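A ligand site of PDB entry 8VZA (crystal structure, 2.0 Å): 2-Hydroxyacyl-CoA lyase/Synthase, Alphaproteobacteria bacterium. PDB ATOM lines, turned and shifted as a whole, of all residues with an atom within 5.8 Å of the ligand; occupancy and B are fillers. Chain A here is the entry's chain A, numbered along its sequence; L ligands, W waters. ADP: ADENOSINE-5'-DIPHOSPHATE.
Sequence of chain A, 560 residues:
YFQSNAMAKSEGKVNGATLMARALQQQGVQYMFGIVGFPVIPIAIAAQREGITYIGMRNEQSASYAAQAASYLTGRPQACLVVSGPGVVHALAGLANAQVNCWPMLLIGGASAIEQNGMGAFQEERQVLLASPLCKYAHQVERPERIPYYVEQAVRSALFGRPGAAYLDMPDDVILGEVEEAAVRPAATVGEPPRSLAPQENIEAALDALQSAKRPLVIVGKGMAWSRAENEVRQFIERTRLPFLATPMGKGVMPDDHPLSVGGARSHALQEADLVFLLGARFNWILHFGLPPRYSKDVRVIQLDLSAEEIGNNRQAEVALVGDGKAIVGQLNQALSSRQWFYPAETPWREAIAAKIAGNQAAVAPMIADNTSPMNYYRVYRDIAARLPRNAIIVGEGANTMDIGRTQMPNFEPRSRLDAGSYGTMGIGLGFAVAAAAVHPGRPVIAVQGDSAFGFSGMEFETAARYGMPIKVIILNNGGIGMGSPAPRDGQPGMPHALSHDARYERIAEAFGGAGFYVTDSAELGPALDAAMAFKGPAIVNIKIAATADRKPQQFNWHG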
ATOM      1  N   VAL A 100     -24.764 -10.072 -35.332  1.00  0.00           N
ATOM      2  CA  VAL A 100     -25.357 -10.684 -34.142  1.00  0.00           C
ATOM      3  C   VAL A 100     -24.585 -10.293 -32.884  1.00  0.00           C
ATOM      4  O   VAL A 100     -25.189 -10.145 -31.811  1.00  0.00           O
ATOM      5  CB  VAL A 100     -25.421 -12.218 -34.296  1.00  0.00           C
ATOM      6  CG1 VAL A 100     -26.009 -12.853 -33.053  1.00  0.00           C
ATOM      7  CG2 VAL A 100     -26.254 -12.590 -35.521  1.00  0.00           C
ATOM      8  N   ASN A 101     -23.274 -10.114 -32.979  1.00  0.00           N
ATOM      9  CA  ASN A 101     -22.472  -9.778 -31.807  1.00  0.00           C
ATOM     10  C   ASN A 101     -22.354  -8.277 -31.565  1.00  0.00           C
ATOM     11  O   ASN A 101     -21.823  -7.880 -30.523  1.00  0.00           O
ATOM     12  CB  ASN A 101     -21.067 -10.388 -31.949  1.00  0.00           C
ATOM     13  CG  ASN A 101     -21.090 -11.898 -31.819  1.00  0.00           C
ATOM     14  OD1 ASN A 101     -21.113 -12.438 -30.719  1.00  0.00           O
ATOM     15  ND2 ASN A 101     -21.089 -12.591 -32.949  1.00  0.00           N
ATOM     16  N   CYS A 102     -22.866  -7.440 -32.473  1.00  0.00           N
ATOM     17  CA  CYS A 102     -22.781  -5.981 -32.365  1.00  0.00           C
ATOM     18  C   CYS A 102     -21.327  -5.506 -32.401  1.00  0.00           C
ATOM     19  O   CYS A 102     -20.941  -4.595 -31.651  1.00  0.00           O
ATOM     20  CB  CYS A 102     -23.503  -5.466 -31.126  1.00  0.00           C
ATOM     21  SG  CYS A 102     -25.247  -5.928 -31.041  1.00  0.00           S
ATOM     22  N   GLY A 161     -23.228   4.371 -32.397  1.00  0.00           N
ATOM     23  CA  GLY A 161     -24.441   3.701 -31.961  1.00  0.00           C
ATOM     24  C   GLY A 161     -24.181   2.242 -31.653  1.00  0.00           C
ATOM     25  O   GLY A 161     -23.109   1.863 -31.170  1.00  0.00           O
ATOM     26  N   ARG A 162     -25.163   1.406 -31.926  1.00  0.00           N
ATOM     27  CA  ARG A 162     -24.964  -0.032 -31.800  1.00  0.00           C
ATOM     28  C   ARG A 162     -24.064  -0.489 -32.940  1.00  0.00           C
ATOM     29  O   ARG A 162     -24.466  -0.376 -34.113  1.00  0.00           O
ATOM     30  CB  ARG A 162     -26.294  -0.775 -31.812  1.00  0.00           C
ATOM     31  CG  ARG A 162     -26.154  -2.280 -31.659  1.00  0.00           C
ATOM     32  CD  ARG A 162     -27.516  -2.961 -31.598  1.00  0.00           C
ATOM     33  NE  ARG A 162     -27.765  -3.561 -30.286  1.00  0.00           N
ATOM     34  CZ  ARG A 162     -28.835  -4.286 -29.984  1.00  0.00           C
ATOM     35  NH1 ARG A 162     -29.796  -4.493 -30.865  1.00  0.00           N
ATOM     36  NH2 ARG A 162     -28.943  -4.812 -28.771  1.00  0.00           N
ATOM     37  N   PRO A 163     -22.862  -0.984 -32.672  1.00  0.00           N
ATOM     38  CA  PRO A 163     -21.923  -1.298 -33.758  1.00  0.00           C
ATOM     39  C   PRO A 163     -22.405  -2.463 -34.617  1.00  0.00           C
ATOM     40  O   PRO A 163     -23.211  -3.291 -34.202  1.00  0.00           O
ATOM     41  CB  PRO A 163     -20.627  -1.659 -33.012  1.00  0.00           C
ATOM     42  CG  PRO A 163     -20.795  -1.116 -31.623  1.00  0.00           C
ATOM     43  CD  PRO A 163     -22.259  -1.217 -31.342  1.00  0.00           C
ATOM     44  N   ARG A 195     -20.899   8.946 -26.533  1.00  0.00           N
ATOM     45  CA  ARG A 195     -21.410   8.354 -25.311  1.00  0.00           C
ATOM     46  C   ARG A 195     -22.617   9.159 -24.844  1.00  0.00           C
ATOM     47  O   ARG A 195     -22.599  10.395 -24.907  1.00  0.00           O
ATOM     48  CB  ARG A 195     -20.325   8.311 -24.224  1.00  0.00           C
ATOM     49  CG  ARG A 195     -19.062   7.531 -24.626  1.00  0.00           C
ATOM     50  CD  ARG A 195     -18.087   7.364 -23.445  1.00  0.00           C
ATOM     51  NE  ARG A 195     -16.806   6.789 -23.834  1.00  0.00           N
ATOM     52  CZ  ARG A 195     -16.516   5.494 -23.837  1.00  0.00           C
ATOM     53  NH1 ARG A 195     -17.411   4.583 -23.495  1.00  0.00           N
ATOM     54  NH2 ARG A 195     -15.291   5.102 -24.185  1.00  0.00           N
ATOM     55  N   VAL A 220     -22.337  -8.924 -16.005  1.00  0.00           N
ATOM     56  CA  VAL A 220     -21.351  -8.149 -16.766  1.00  0.00           C
ATOM     57  C   VAL A 220     -21.221  -8.756 -18.157  1.00  0.00           C
ATOM     58  O   VAL A 220     -20.661  -9.842 -18.323  1.00  0.00           O
ATOM     59  CB  VAL A 220     -19.997  -8.131 -16.046  1.00  0.00           C
ATOM     60  CG1 VAL A 220     -18.994  -7.272 -16.824  1.00  0.00           C
ATOM     61  CG2 VAL A 220     -20.137  -7.631 -14.604  1.00  0.00           C
ATOM     62  N   GLY A 221     -21.711  -8.037 -19.175  1.00  0.00           N
ATOM     63  CA  GLY A 221     -21.694  -8.515 -20.534  1.00  0.00           C
ATOM     64  C   GLY A 221     -20.617  -7.843 -21.374  1.00  0.00           C
ATOM     65  O   GLY A 221     -20.084  -6.798 -21.010  1.00  0.00           O
ATOM     66  N   LYS A 222     -20.318  -8.464 -22.522  1.00  0.00           N
ATOM     67  CA  LYS A 222     -19.265  -7.960 -23.392  1.00  0.00           C
ATOM     68  C   LYS A 222     -19.573  -6.575 -23.956  1.00  0.00           C
ATOM     69  O   LYS A 222     -18.679  -5.943 -24.536  1.00  0.00           O
ATOM     70  CB  LYS A 222     -18.975  -8.947 -24.526  1.00  0.00           C
ATOM     71  CG  LYS A 222     -20.163  -9.275 -25.444  1.00  0.00           C
ATOM     72  CD  LYS A 222     -19.702 -10.195 -26.566  1.00  0.00           C
ATOM     73  CE  LYS A 222     -20.836 -11.012 -27.185  1.00  0.00           C
ATOM     74  NZ  LYS A 222     -21.657 -10.230 -28.138  1.00  0.00           N
ATOM     75  N   GLY A 223     -20.809  -6.085 -23.815  1.00  0.00           N
ATOM     76  CA  GLY A 223     -21.065  -4.685 -24.111  1.00  0.00           C
ATOM     77  C   GLY A 223     -20.203  -3.753 -23.275  1.00  0.00           C
ATOM     78  O   GLY A 223     -19.733  -2.722 -23.763  1.00  0.00           O
ATOM     79  N   MET A 224     -19.959  -4.110 -22.010  1.00  0.00           N
ATOM     80  CA  MET A 224     -19.057  -3.314 -21.179  1.00  0.00           C
ATOM     81  C   MET A 224     -17.621  -3.436 -21.664  1.00  0.00           C
ATOM     82  O   MET A 224     -16.857  -2.468 -21.605  1.00  0.00           O
ATOM     83  CB  MET A 224     -19.169  -3.741 -19.717  1.00  0.00           C
ATOM     84  CG  MET A 224     -20.583  -3.733 -19.157  1.00  0.00           C
ATOM     85  SD  MET A 224     -21.424  -2.162 -19.362  1.00  0.00           S
ATOM     86  CE  MET A 224     -20.490  -1.095 -18.286  1.00  0.00           C
ATOM     87  N   TRP A 226     -16.712  -3.851 -24.796  1.00  0.00           N
ATOM     88  CA  TRP A 226     -16.594  -3.032 -25.996  1.00  0.00           C
ATOM     89  C   TRP A 226     -16.586  -1.546 -25.647  1.00  0.00           C
ATOM     90  O   TRP A 226     -15.872  -0.755 -26.284  1.00  0.00           O
ATOM     91  CB  TRP A 226     -17.731  -3.347 -26.976  1.00  0.00           C
ATOM     92  CG  TRP A 226     -17.927  -2.247 -27.959  1.00  0.00           C
ATOM     93  CD1 TRP A 226     -18.933  -1.324 -27.953  1.00  0.00           C
ATOM     94  CD2 TRP A 226     -17.085  -1.929 -29.068  1.00  0.00           C
ATOM     95  NE1 TRP A 226     -18.772  -0.450 -29.012  1.00  0.00           N
ATOM     96  CE2 TRP A 226     -17.648  -0.797 -29.699  1.00  0.00           C
ATOM     97  CE3 TRP A 226     -15.916  -2.488 -29.587  1.00  0.00           C
ATOM     98  CZ2 TRP A 226     -17.073  -0.226 -30.827  1.00  0.00           C
ATOM     99  CZ3 TRP A 226     -15.344  -1.910 -30.709  1.00  0.00           C
ATOM    100  CH2 TRP A 226     -15.919  -0.790 -31.312  1.00  0.00           C
ATOM    101  N   SER A 227     -17.349  -1.150 -24.636  1.00  0.00           N
ATOM    102  CA  SER A 227     -17.387   0.243 -24.203  1.00  0.00           C
ATOM    103  C   SER A 227     -16.117   0.672 -23.466  1.00  0.00           C
ATOM    104  O   SER A 227     -16.007   1.865 -23.145  1.00  0.00           O
ATOM    105  CB  SER A 227     -18.609   0.462 -23.306  1.00  0.00           C
ATOM    106  OG  SER A 227     -18.712   1.803 -22.852  1.00  0.00           O
ATOM    107  N   THR A 247     -20.702 -12.866 -18.386  1.00  0.00           N
ATOM    108  CA  THR A 247     -21.095 -13.648 -19.558  1.00  0.00           C
ATOM    109  C   THR A 247     -19.841 -14.274 -20.155  1.00  0.00           C
ATOM    110  O   THR A 247     -18.721 -13.985 -19.725  1.00  0.00           O
ATOM    111  CB  THR A 247     -21.831 -12.760 -20.560  1.00  0.00           C
ATOM    112  OG1 THR A 247     -20.939 -11.739 -21.034  1.00  0.00           O
ATOM    113  CG2 THR A 247     -23.044 -12.107 -19.909  1.00  0.00           C
ATOM    114  N   PRO A 248     -19.992 -15.170 -21.158  1.00  0.00           N
ATOM    115  CA  PRO A 248     -18.786 -15.786 -21.740  1.00  0.00           C
ATOM    116  C   PRO A 248     -17.714 -14.815 -22.197  1.00  0.00           C
ATOM    117  O   PRO A 248     -16.542 -14.974 -21.819  1.00  0.00           O
ATOM    118  CB  PRO A 248     -19.362 -16.605 -22.901  1.00  0.00           C
ATOM    119  CG  PRO A 248     -20.674 -17.040 -22.392  1.00  0.00           C
ATOM    120  CD  PRO A 248     -21.213 -15.857 -21.612  1.00  0.00           C
ATOM    121  N   MET A 249     -18.052 -13.818 -23.006  1.00  0.00           N
ATOM    122  CA  MET A 249     -17.052 -12.854 -23.437  1.00  0.00           C
ATOM    123  C   MET A 249     -17.045 -11.590 -22.598  1.00  0.00           C
ATOM    124  O   MET A 249     -16.156 -10.745 -22.767  1.00  0.00           O
ATOM    125  CB  MET A 249     -17.220 -12.524 -24.925  1.00  0.00           C
ATOM    126  CG  MET A 249     -16.510 -13.538 -25.814  1.00  0.00           C
ATOM    127  SD  MET A 249     -16.301 -13.040 -27.532  1.00  0.00           S
ATOM    128  CE  MET A 249     -18.000 -13.137 -28.090  1.00  0.00           C
ATOM    129  N   GLY A 250     -17.995 -11.445 -21.675  1.00  0.00           N
ATOM    130  CA  GLY A 250     -17.846 -10.463 -20.632  1.00  0.00           C
ATOM    131  C   GLY A 250     -16.751 -10.788 -19.633  1.00  0.00           C
ATOM    132  O   GLY A 250     -16.351  -9.894 -18.870  1.00  0.00           O
ATOM    133  N   GLY A 280     -24.675  -4.181 -20.154  1.00  0.00           N
ATOM    134  CA  GLY A 280     -24.289  -4.493 -21.518  1.00  0.00           C
ATOM    135  C   GLY A 280     -24.423  -5.962 -21.830  1.00  0.00           C
ATOM    136  O   GLY A 280     -23.497  -6.574 -22.363  1.00  0.00           O
ATOM    137  N   ALA A 281     -25.571  -6.549 -21.489  1.00  0.00           N
ATOM    138  CA  ALA A 281     -25.859  -7.946 -21.748  1.00  0.00           C
ATOM    139  C   ALA A 281     -27.324  -8.090 -22.108  1.00  0.00           C
ATOM    140  O   ALA A 281     -28.190  -7.460 -21.498  1.00  0.00           O
ATOM    141  CB  ALA A 281     -25.537  -8.829 -20.540  1.00  0.00           C
ATOM    142  N   ARG A 282     -27.611  -8.938 -23.104  1.00  0.00           N
ATOM    143  CA  ARG A 282     -28.971  -9.137 -23.565  1.00  0.00           C
ATOM    144  C   ARG A 282     -29.600 -10.369 -22.939  1.00  0.00           C
ATOM    145  O   ARG A 282     -28.922 -11.347 -22.616  1.00  0.00           O
ATOM    146  CB  ARG A 282     -29.009  -9.264 -25.092  1.00  0.00           C
ATOM    147  CG  ARG A 282     -28.638  -7.987 -25.819  1.00  0.00           C
ATOM    148  CD  ARG A 282     -28.547  -8.233 -27.313  1.00  0.00           C
ATOM    149  NE  ARG A 282     -27.374  -9.040 -27.654  1.00  0.00           N
ATOM    150  CZ  ARG A 282     -27.073  -9.445 -28.883  1.00  0.00           C
ATOM    151  NH1 ARG A 282     -27.843  -9.169 -29.918  1.00  0.00           N
ATOM    152  NH2 ARG A 282     -25.952 -10.135 -29.075  1.00  0.00           N
ATOM    153  N   ASN A 284     -31.027 -12.735 -24.315  1.00  0.00           N
ATOM    154  CA  ASN A 284     -31.157 -13.706 -25.381  1.00  0.00           C
ATOM    155  C   ASN A 284     -30.841 -15.092 -24.811  1.00  0.00           C
ATOM    156  O   ASN A 284     -30.849 -15.277 -23.588  1.00  0.00           O
ATOM    157  CB  ASN A 284     -30.243 -13.308 -26.562  1.00  0.00           C
ATOM    158  CG  ASN A 284     -28.782 -13.307 -26.202  1.00  0.00           C
ATOM    159  OD1 ASN A 284     -28.410 -13.565 -25.059  1.00  0.00           O
ATOM    160  ND2 ASN A 284     -27.931 -13.029 -27.184  1.00  0.00           N
ATOM    161  N   ILE A 286     -28.161 -16.726 -24.356  1.00  0.00           N
ATOM    162  CA  ILE A 286     -26.983 -16.842 -23.492  1.00  0.00           C
ATOM    163  C   ILE A 286     -27.359 -16.612 -22.030  1.00  0.00           C
ATOM    164  O   ILE A 286     -26.826 -17.274 -21.121  1.00  0.00           O
ATOM    165  CB  ILE A 286     -25.870 -15.878 -23.954  1.00  0.00           C
ATOM    166  CG1 ILE A 286     -24.958 -16.577 -24.973  1.00  0.00           C
ATOM    167  CG2 ILE A 286     -25.063 -15.342 -22.769  1.00  0.00           C
ATOM    168  CD1 ILE A 286     -23.891 -15.682 -25.575  1.00  0.00           C
ATOM    169  N   LEU A 287     -28.286 -15.686 -21.779  1.00  0.00           N
ATOM    170  CA  LEU A 287     -28.806 -15.464 -20.431  1.00  0.00           C
ATOM    171  C   LEU A 287     -30.174 -16.094 -20.231  1.00  0.00           C
ATOM    172  O   LEU A 287     -30.891 -15.713 -19.299  1.00  0.00           O
ATOM    173  CB  LEU A 287     -28.848 -13.961 -20.131  1.00  0.00           C
ATOM    174  CG  LEU A 287     -27.492 -13.327 -19.783  1.00  0.00           C
ATOM    175  CD1 LEU A 287     -27.652 -11.852 -19.452  1.00  0.00           C
ATOM    176  CD2 LEU A 287     -26.816 -14.076 -18.632  1.00  0.00           C
ATOM    177  N   LEU A 304     -28.947  -1.830 -18.503  1.00  0.00           N
ATOM    178  CA  LEU A 304     -28.106  -0.840 -19.169  1.00  0.00           C
ATOM    179  C   LEU A 304     -27.788  -1.340 -20.577  1.00  0.00           C
ATOM    180  O   LEU A 304     -27.116  -2.361 -20.739  1.00  0.00           O
ATOM    181  CB  LEU A 304     -26.813  -0.610 -18.381  1.00  0.00           C
ATOM    182  CG  LEU A 304     -25.985   0.658 -18.590  1.00  0.00           C
ATOM    183  CD1 LEU A 304     -24.870   0.725 -17.548  1.00  0.00           C
ATOM    184  CD2 LEU A 304     -25.383   0.766 -19.991  1.00  0.00           C
ATOM    185  N   ASP A 305     -28.251  -0.612 -21.576  1.00  0.00           N
ATOM    186  CA  ASP A 305     -27.920  -0.956 -22.959  1.00  0.00           C
ATOM    187  C   ASP A 305     -27.897   0.317 -23.784  1.00  0.00           C
ATOM    188  O   ASP A 305     -28.618   1.275 -23.508  1.00  0.00           O
ATOM    189  CB  ASP A 305     -28.914  -1.967 -23.545  1.00  0.00           C
ATOM    190  CG  ASP A 305     -28.354  -2.710 -24.750  1.00  0.00           C
ATOM    191  OD1 ASP A 305     -27.867  -2.051 -25.707  1.00  0.00           O
ATOM    192  OD2 ASP A 305     -28.389  -3.957 -24.734  1.00  0.00           O
ATOM    193  N   LEU A 306     -27.037   0.313 -24.801  1.00  0.00           N
ATOM    194  CA  LEU A 306     -26.960   1.461 -25.694  1.00  0.00           C
ATOM    195  C   LEU A 306     -28.166   1.532 -26.617  1.00  0.00           C
ATOM    196  O   LEU A 306     -28.545   2.612 -27.069  1.00  0.00           O
ATOM    197  CB  LEU A 306     -25.659   1.412 -26.484  1.00  0.00           C
ATOM    198  CG  LEU A 306     -25.352   2.509 -27.491  1.00  0.00           C
ATOM    199  CD1 LEU A 306     -25.514   3.895 -26.883  1.00  0.00           C
ATOM    200  CD2 LEU A 306     -23.932   2.304 -27.994  1.00  0.00           C
ATOM    201  N   SER A 307     -28.784   0.380 -26.897  1.00  0.00           N
ATOM    202  CA  SER A 307     -29.906   0.298 -27.835  1.00  0.00           C
ATOM    203  C   SER A 307     -31.215   0.371 -27.046  1.00  0.00           C
ATOM    204  O   SER A 307     -31.515  -0.531 -26.263  1.00  0.00           O
ATOM    205  CB  SER A 307     -29.823  -0.991 -28.648  1.00  0.00           C
ATOM    206  OG  SER A 307     -30.928  -1.127 -29.540  1.00  0.00           O
ATOM    207  N   GLU A 310     -33.674  -2.629 -27.315  1.00  0.00           N
ATOM    208  CA  GLU A 310     -33.388  -3.838 -26.560  1.00  0.00           C
ATOM    209  C   GLU A 310     -34.037  -3.850 -25.189  1.00  0.00           C
ATOM    210  O   GLU A 310     -34.274  -4.934 -24.636  1.00  0.00           O
ATOM    211  CB  GLU A 310     -31.874  -4.011 -26.413  1.00  0.00           C
ATOM    212  CG  GLU A 310     -31.444  -5.375 -25.904  1.00  0.00           C
ATOM    213  CD  GLU A 310     -31.694  -6.482 -26.917  1.00  0.00           C
ATOM    214  OE1 GLU A 310     -31.539  -6.225 -28.129  1.00  0.00           O
ATOM    215  OE2 GLU A 310     -32.046  -7.607 -26.506  1.00  0.00           O
ATOM    216  N   GLY A 323     -27.873   4.218 -22.672  1.00  0.00           N
ATOM    217  CA  GLY A 323     -26.706   5.046 -22.907  1.00  0.00           C
ATOM    218  C   GLY A 323     -25.465   4.187 -22.951  1.00  0.00           C
ATOM    219  O   GLY A 323     -25.535   2.962 -23.000  1.00  0.00           O
ATOM    220  N   ASP A 324     -24.323   4.865 -22.928  1.00  0.00           N
ATOM    221  CA  ASP A 324     -23.034   4.191 -22.970  1.00  0.00           C
ATOM    222  C   ASP A 324     -22.721   3.539 -21.623  1.00  0.00           C
ATOM    223  O   ASP A 324     -22.944   4.125 -20.564  1.00  0.00           O
ATOM    224  CB  ASP A 324     -21.924   5.175 -23.339  1.00  0.00           C
ATOM    225  CG  ASP A 324     -20.551   4.534 -23.315  1.00  0.00           C
ATOM    226  OD1 ASP A 324     -20.304   3.638 -24.137  1.00  0.00           O
ATOM    227  OD2 ASP A 324     -19.728   4.927 -22.454  1.00  0.00           O
ATOM    228  N   GLY A 325     -22.146   2.333 -21.691  1.00  0.00           N
ATOM    229  CA  GLY A 325     -21.815   1.599 -20.471  1.00  0.00           C
ATOM    230  C   GLY A 325     -20.835   2.336 -19.574  1.00  0.00           C
ATOM    231  O   GLY A 325     -21.056   2.466 -18.374  1.00  0.00           O
ATOM    232  N   LYS A 326     -19.732   2.820 -20.148  1.00  0.00           N
ATOM    233  CA  LYS A 326     -18.743   3.563 -19.361  1.00  0.00           C
ATOM    234  C   LYS A 326     -19.343   4.832 -18.779  1.00  0.00           C
ATOM    235  O   LYS A 326     -19.081   5.193 -17.631  1.00  0.00           O
ATOM    236  CB  LYS A 326     -17.527   3.899 -20.221  1.00  0.00           C
ATOM    237  CG  LYS A 326     -16.409   4.617 -19.476  1.00  0.00           C
ATOM    238  CD  LYS A 326     -15.202   4.811 -20.377  1.00  0.00           C
ATOM    239  CE  LYS A 326     -14.003   5.333 -19.590  1.00  0.00           C
ATOM    240  NZ  LYS A 326     -12.788   5.496 -20.428  1.00  0.00           N
ATOM    241  N   SER A 422     -22.429 -14.946 -29.769  1.00  0.00           N
ATOM    242  CA  SER A 422     -23.891 -14.944 -29.730  1.00  0.00           C
ATOM    243  C   SER A 422     -24.518 -15.724 -30.881  1.00  0.00           C
ATOM    244  O   SER A 422     -25.723 -15.988 -30.829  1.00  0.00           O
ATOM    245  CB  SER A 422     -24.409 -13.503 -29.757  1.00  0.00           C
ATOM    246  OG  SER A 422     -23.699 -12.678 -28.852  1.00  0.00           O
HETATM  247  PB  ADP L   1     -23.226 -11.076 -23.849  1.00  0.00           P
HETATM  248  O1B ADP L   1     -23.192 -12.181 -24.882  1.00  0.00           O
HETATM  249  O2B ADP L   1     -24.445 -11.102 -22.971  1.00  0.00           O
HETATM  250  O3B ADP L   1     -21.916 -10.892 -23.112  1.00  0.00           O
HETATM  251  PA  ADP L   1     -24.527  -9.412 -25.772  1.00  0.00           P
HETATM  252  O1A ADP L   1     -23.896  -9.432 -27.144  1.00  0.00           O
HETATM  253  O2A ADP L   1     -25.770 -10.218 -25.499  1.00  0.00           O
HETATM  254  O3A ADP L   1     -23.368  -9.714 -24.685  1.00  0.00           O
HETATM  255  O5' ADP L   1     -24.884  -7.892 -25.390  1.00  0.00           O
HETATM  256  C5' ADP L   1     -24.141  -6.806 -25.920  1.00  0.00           C
HETATM  257  C4' ADP L   1     -24.989  -5.555 -25.751  1.00  0.00           C
HETATM  258  O4' ADP L   1     -24.153  -4.453 -25.418  1.00  0.00           O
HETATM  259  C3' ADP L   1     -25.757  -5.198 -27.016  1.00  0.00           C
HETATM  260  O3' ADP L   1     -27.159  -5.238 -26.751  1.00  0.00           O
HETATM  261  C2' ADP L   1     -25.354  -3.774 -27.349  1.00  0.00           C
HETATM  262  O2' ADP L   1     -26.486  -2.953 -27.670  1.00  0.00           O
HETATM  263  C1' ADP L   1     -24.699  -3.303 -26.066  1.00  0.00           C
HETATM  264  N9  ADP L   1     -23.666  -2.283 -26.292  1.00  0.00           N
HETATM  265  C8  ADP L   1     -22.887  -2.112 -27.375  1.00  0.00           C
HETATM  266  N7  ADP L   1     -22.070  -1.027 -27.204  1.00  0.00           N
HETATM  267  C5  ADP L   1     -22.341  -0.491 -25.998  1.00  0.00           C
HETATM  268  C6  ADP L   1     -21.866   0.654 -25.185  1.00  0.00           C
HETATM  269  N6  ADP L   1     -20.884   1.477 -25.646  1.00  0.00           N
HETATM  270  N1  ADP L   1     -22.437   0.845 -23.978  1.00  0.00           N
HETATM  271  C2  ADP L   1     -23.403   0.040 -23.500  1.00  0.00           C
HETATM  272  N3  ADP L   1     -23.891  -1.017 -24.173  1.00  0.00           N
HETATM  273  C4  ADP L   1     -23.407  -1.321 -25.413  1.00  0.00           C
HETATM  274  O   HOH W   1     -26.510 -12.487 -23.028  1.00  0.00           O
HETATM  275  O   HOH W   2     -25.210 -12.425 -26.624  1.00  0.00           O
HETATM  276  O   HOH W   3     -20.821  -3.458 -29.134  1.00  0.00           O
HETATM  277  O   HOH W   4     -20.608 -13.362 -23.966  1.00  0.00           O
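Water W1 lies within hydrogen-bond range of an oxygen (O2B) of the ligand (2.5 Å), the backbone carbonyl oxygen of Arg 282 (2.7 Å) and the side-chain amide oxygen of Asn 284 (3.0 Å). Water W2 lies within hydrogen-bond range of an oxygen (O2A) of the ligand (2.5 Å), the side-chain hydroxyl of Ser 422 (2.7 Å), the side-chain amide nitrogen of Asn 284 (2.8 Å) and the guanidinium group of Arg 282 (3.4 Å). Water W4 lies within hydrogen-bond range of the backbone NH of Met 249, an oxygen (O3B) of the ligand and the side-chain hydroxyl of Thr 247. Water W3 lies within hydrogen-bond range of O of Cys 102 (2.8 Å) and N7 of the ligand (3.3 Å).
The side-chain hydroxyl (OG1) of Thr 247 is in hydrogen-bond range of the backbone NH (N) of Gly 250, at 3.0 Å. The backbone NH (N) of Thr 247 is in hydrogen-bond range of the backbone carbonyl oxygen (O) of Val 220, at 3.0 Å. The side-chain carboxylate of Asp 324 lies within hydrogen-bond range of the backbone NH of Lys 326, 3.1 Å away. The side-chain carboxylate of Asp 324 is in salt-bridge range of the guanidinium group of Arg 195, at 2.6 Å. The guanidinium group (NH2) of Arg 162 lies within salt-bridge range of the side-chain carboxylate (OE1) of Glu 310, at 3.0 Å. The backbone NH of Gly 223 lies within hydrogen-bond range of the backbone carbonyl oxygen of Gly 280. The backbone NH of Ile 286 sits close to the side-chain amide oxygen of Asn 284 (3.2 Å). The backbone NH (N) of Ser 422 is in hydrogen-bond range of the side-chain amide oxygen (OD1) of Asn 101, at 3.0 Å.
Gly 221 touches the ligand (CA to O3B, 3.5 Å). Gly 223 touches the ligand. CD1 of Trp 226 touches N7 of the ligand, 3.2 Å away. CB of Ser 227 touches N6 of the ligand (3.4 Å). O of Gly 280 touches O5' of the ligand, 3.6 Å away. CB of Ala 281 touches O2B of the ligand, at 3.5 Å. Asn 284 touches the ligand. Ile 286 touches the ligand (CD1 to O1B, 3.6 Å). Ser 307 touches the ligand. O of Gly 323 touches C2 of the ligand, at 3.7 Å. OG of Ser 422 touches O1A of the ligand, 3.7 Å away. Hydrophobic or aromatic side chains that line the ligand: Trp 226, Ala 281, Ile 286 and Leu 306. Of the 34 residues printed, 19 come within 4 Å of the ligand. The nearest printed residue that does not touch the ligand is Leu 304 (4.1 Å).
The side-chain hydroxyl of Thr 247 is in hydrogen-bond range of an oxygen (O3B) of the ligand (2.4 Å). An oxygen (O2') of the ligand lies within hydrogen-bond range of the side-chain carboxylate of Asp 305. An oxygen (O3B) of the ligand is in hydrogen-bond range of the backbone NH (N) of Lys 222, 3.0 Å away. O1A of the ligand is in salt-bridge range of NZ of Lys 222, at 2.6 Å. The side-chain carboxylate (OD1) of Asp 324 sits at hydrogen-bond distance from a nitrogen (N6) of the ligand, at 2.7 Å. The guanidinium group (NH2) of Arg 162 is in hydrogen-bond range of an oxygen (O3') of the ligand. The backbone NH (N) of Gly 325 lies within hydrogen-bond range of a nitrogen (N1) of the ligand, at 2.7 Å. N of Arg 282 lies within hydrogen-bond range of O2A of the ligand, at 3.3 Å. NH2 of Arg 282 lies within salt-bridge range of O1A of the ligand (2.9 Å). N3 of the ligand lies within hydrogen-bond range of N of Leu 306.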
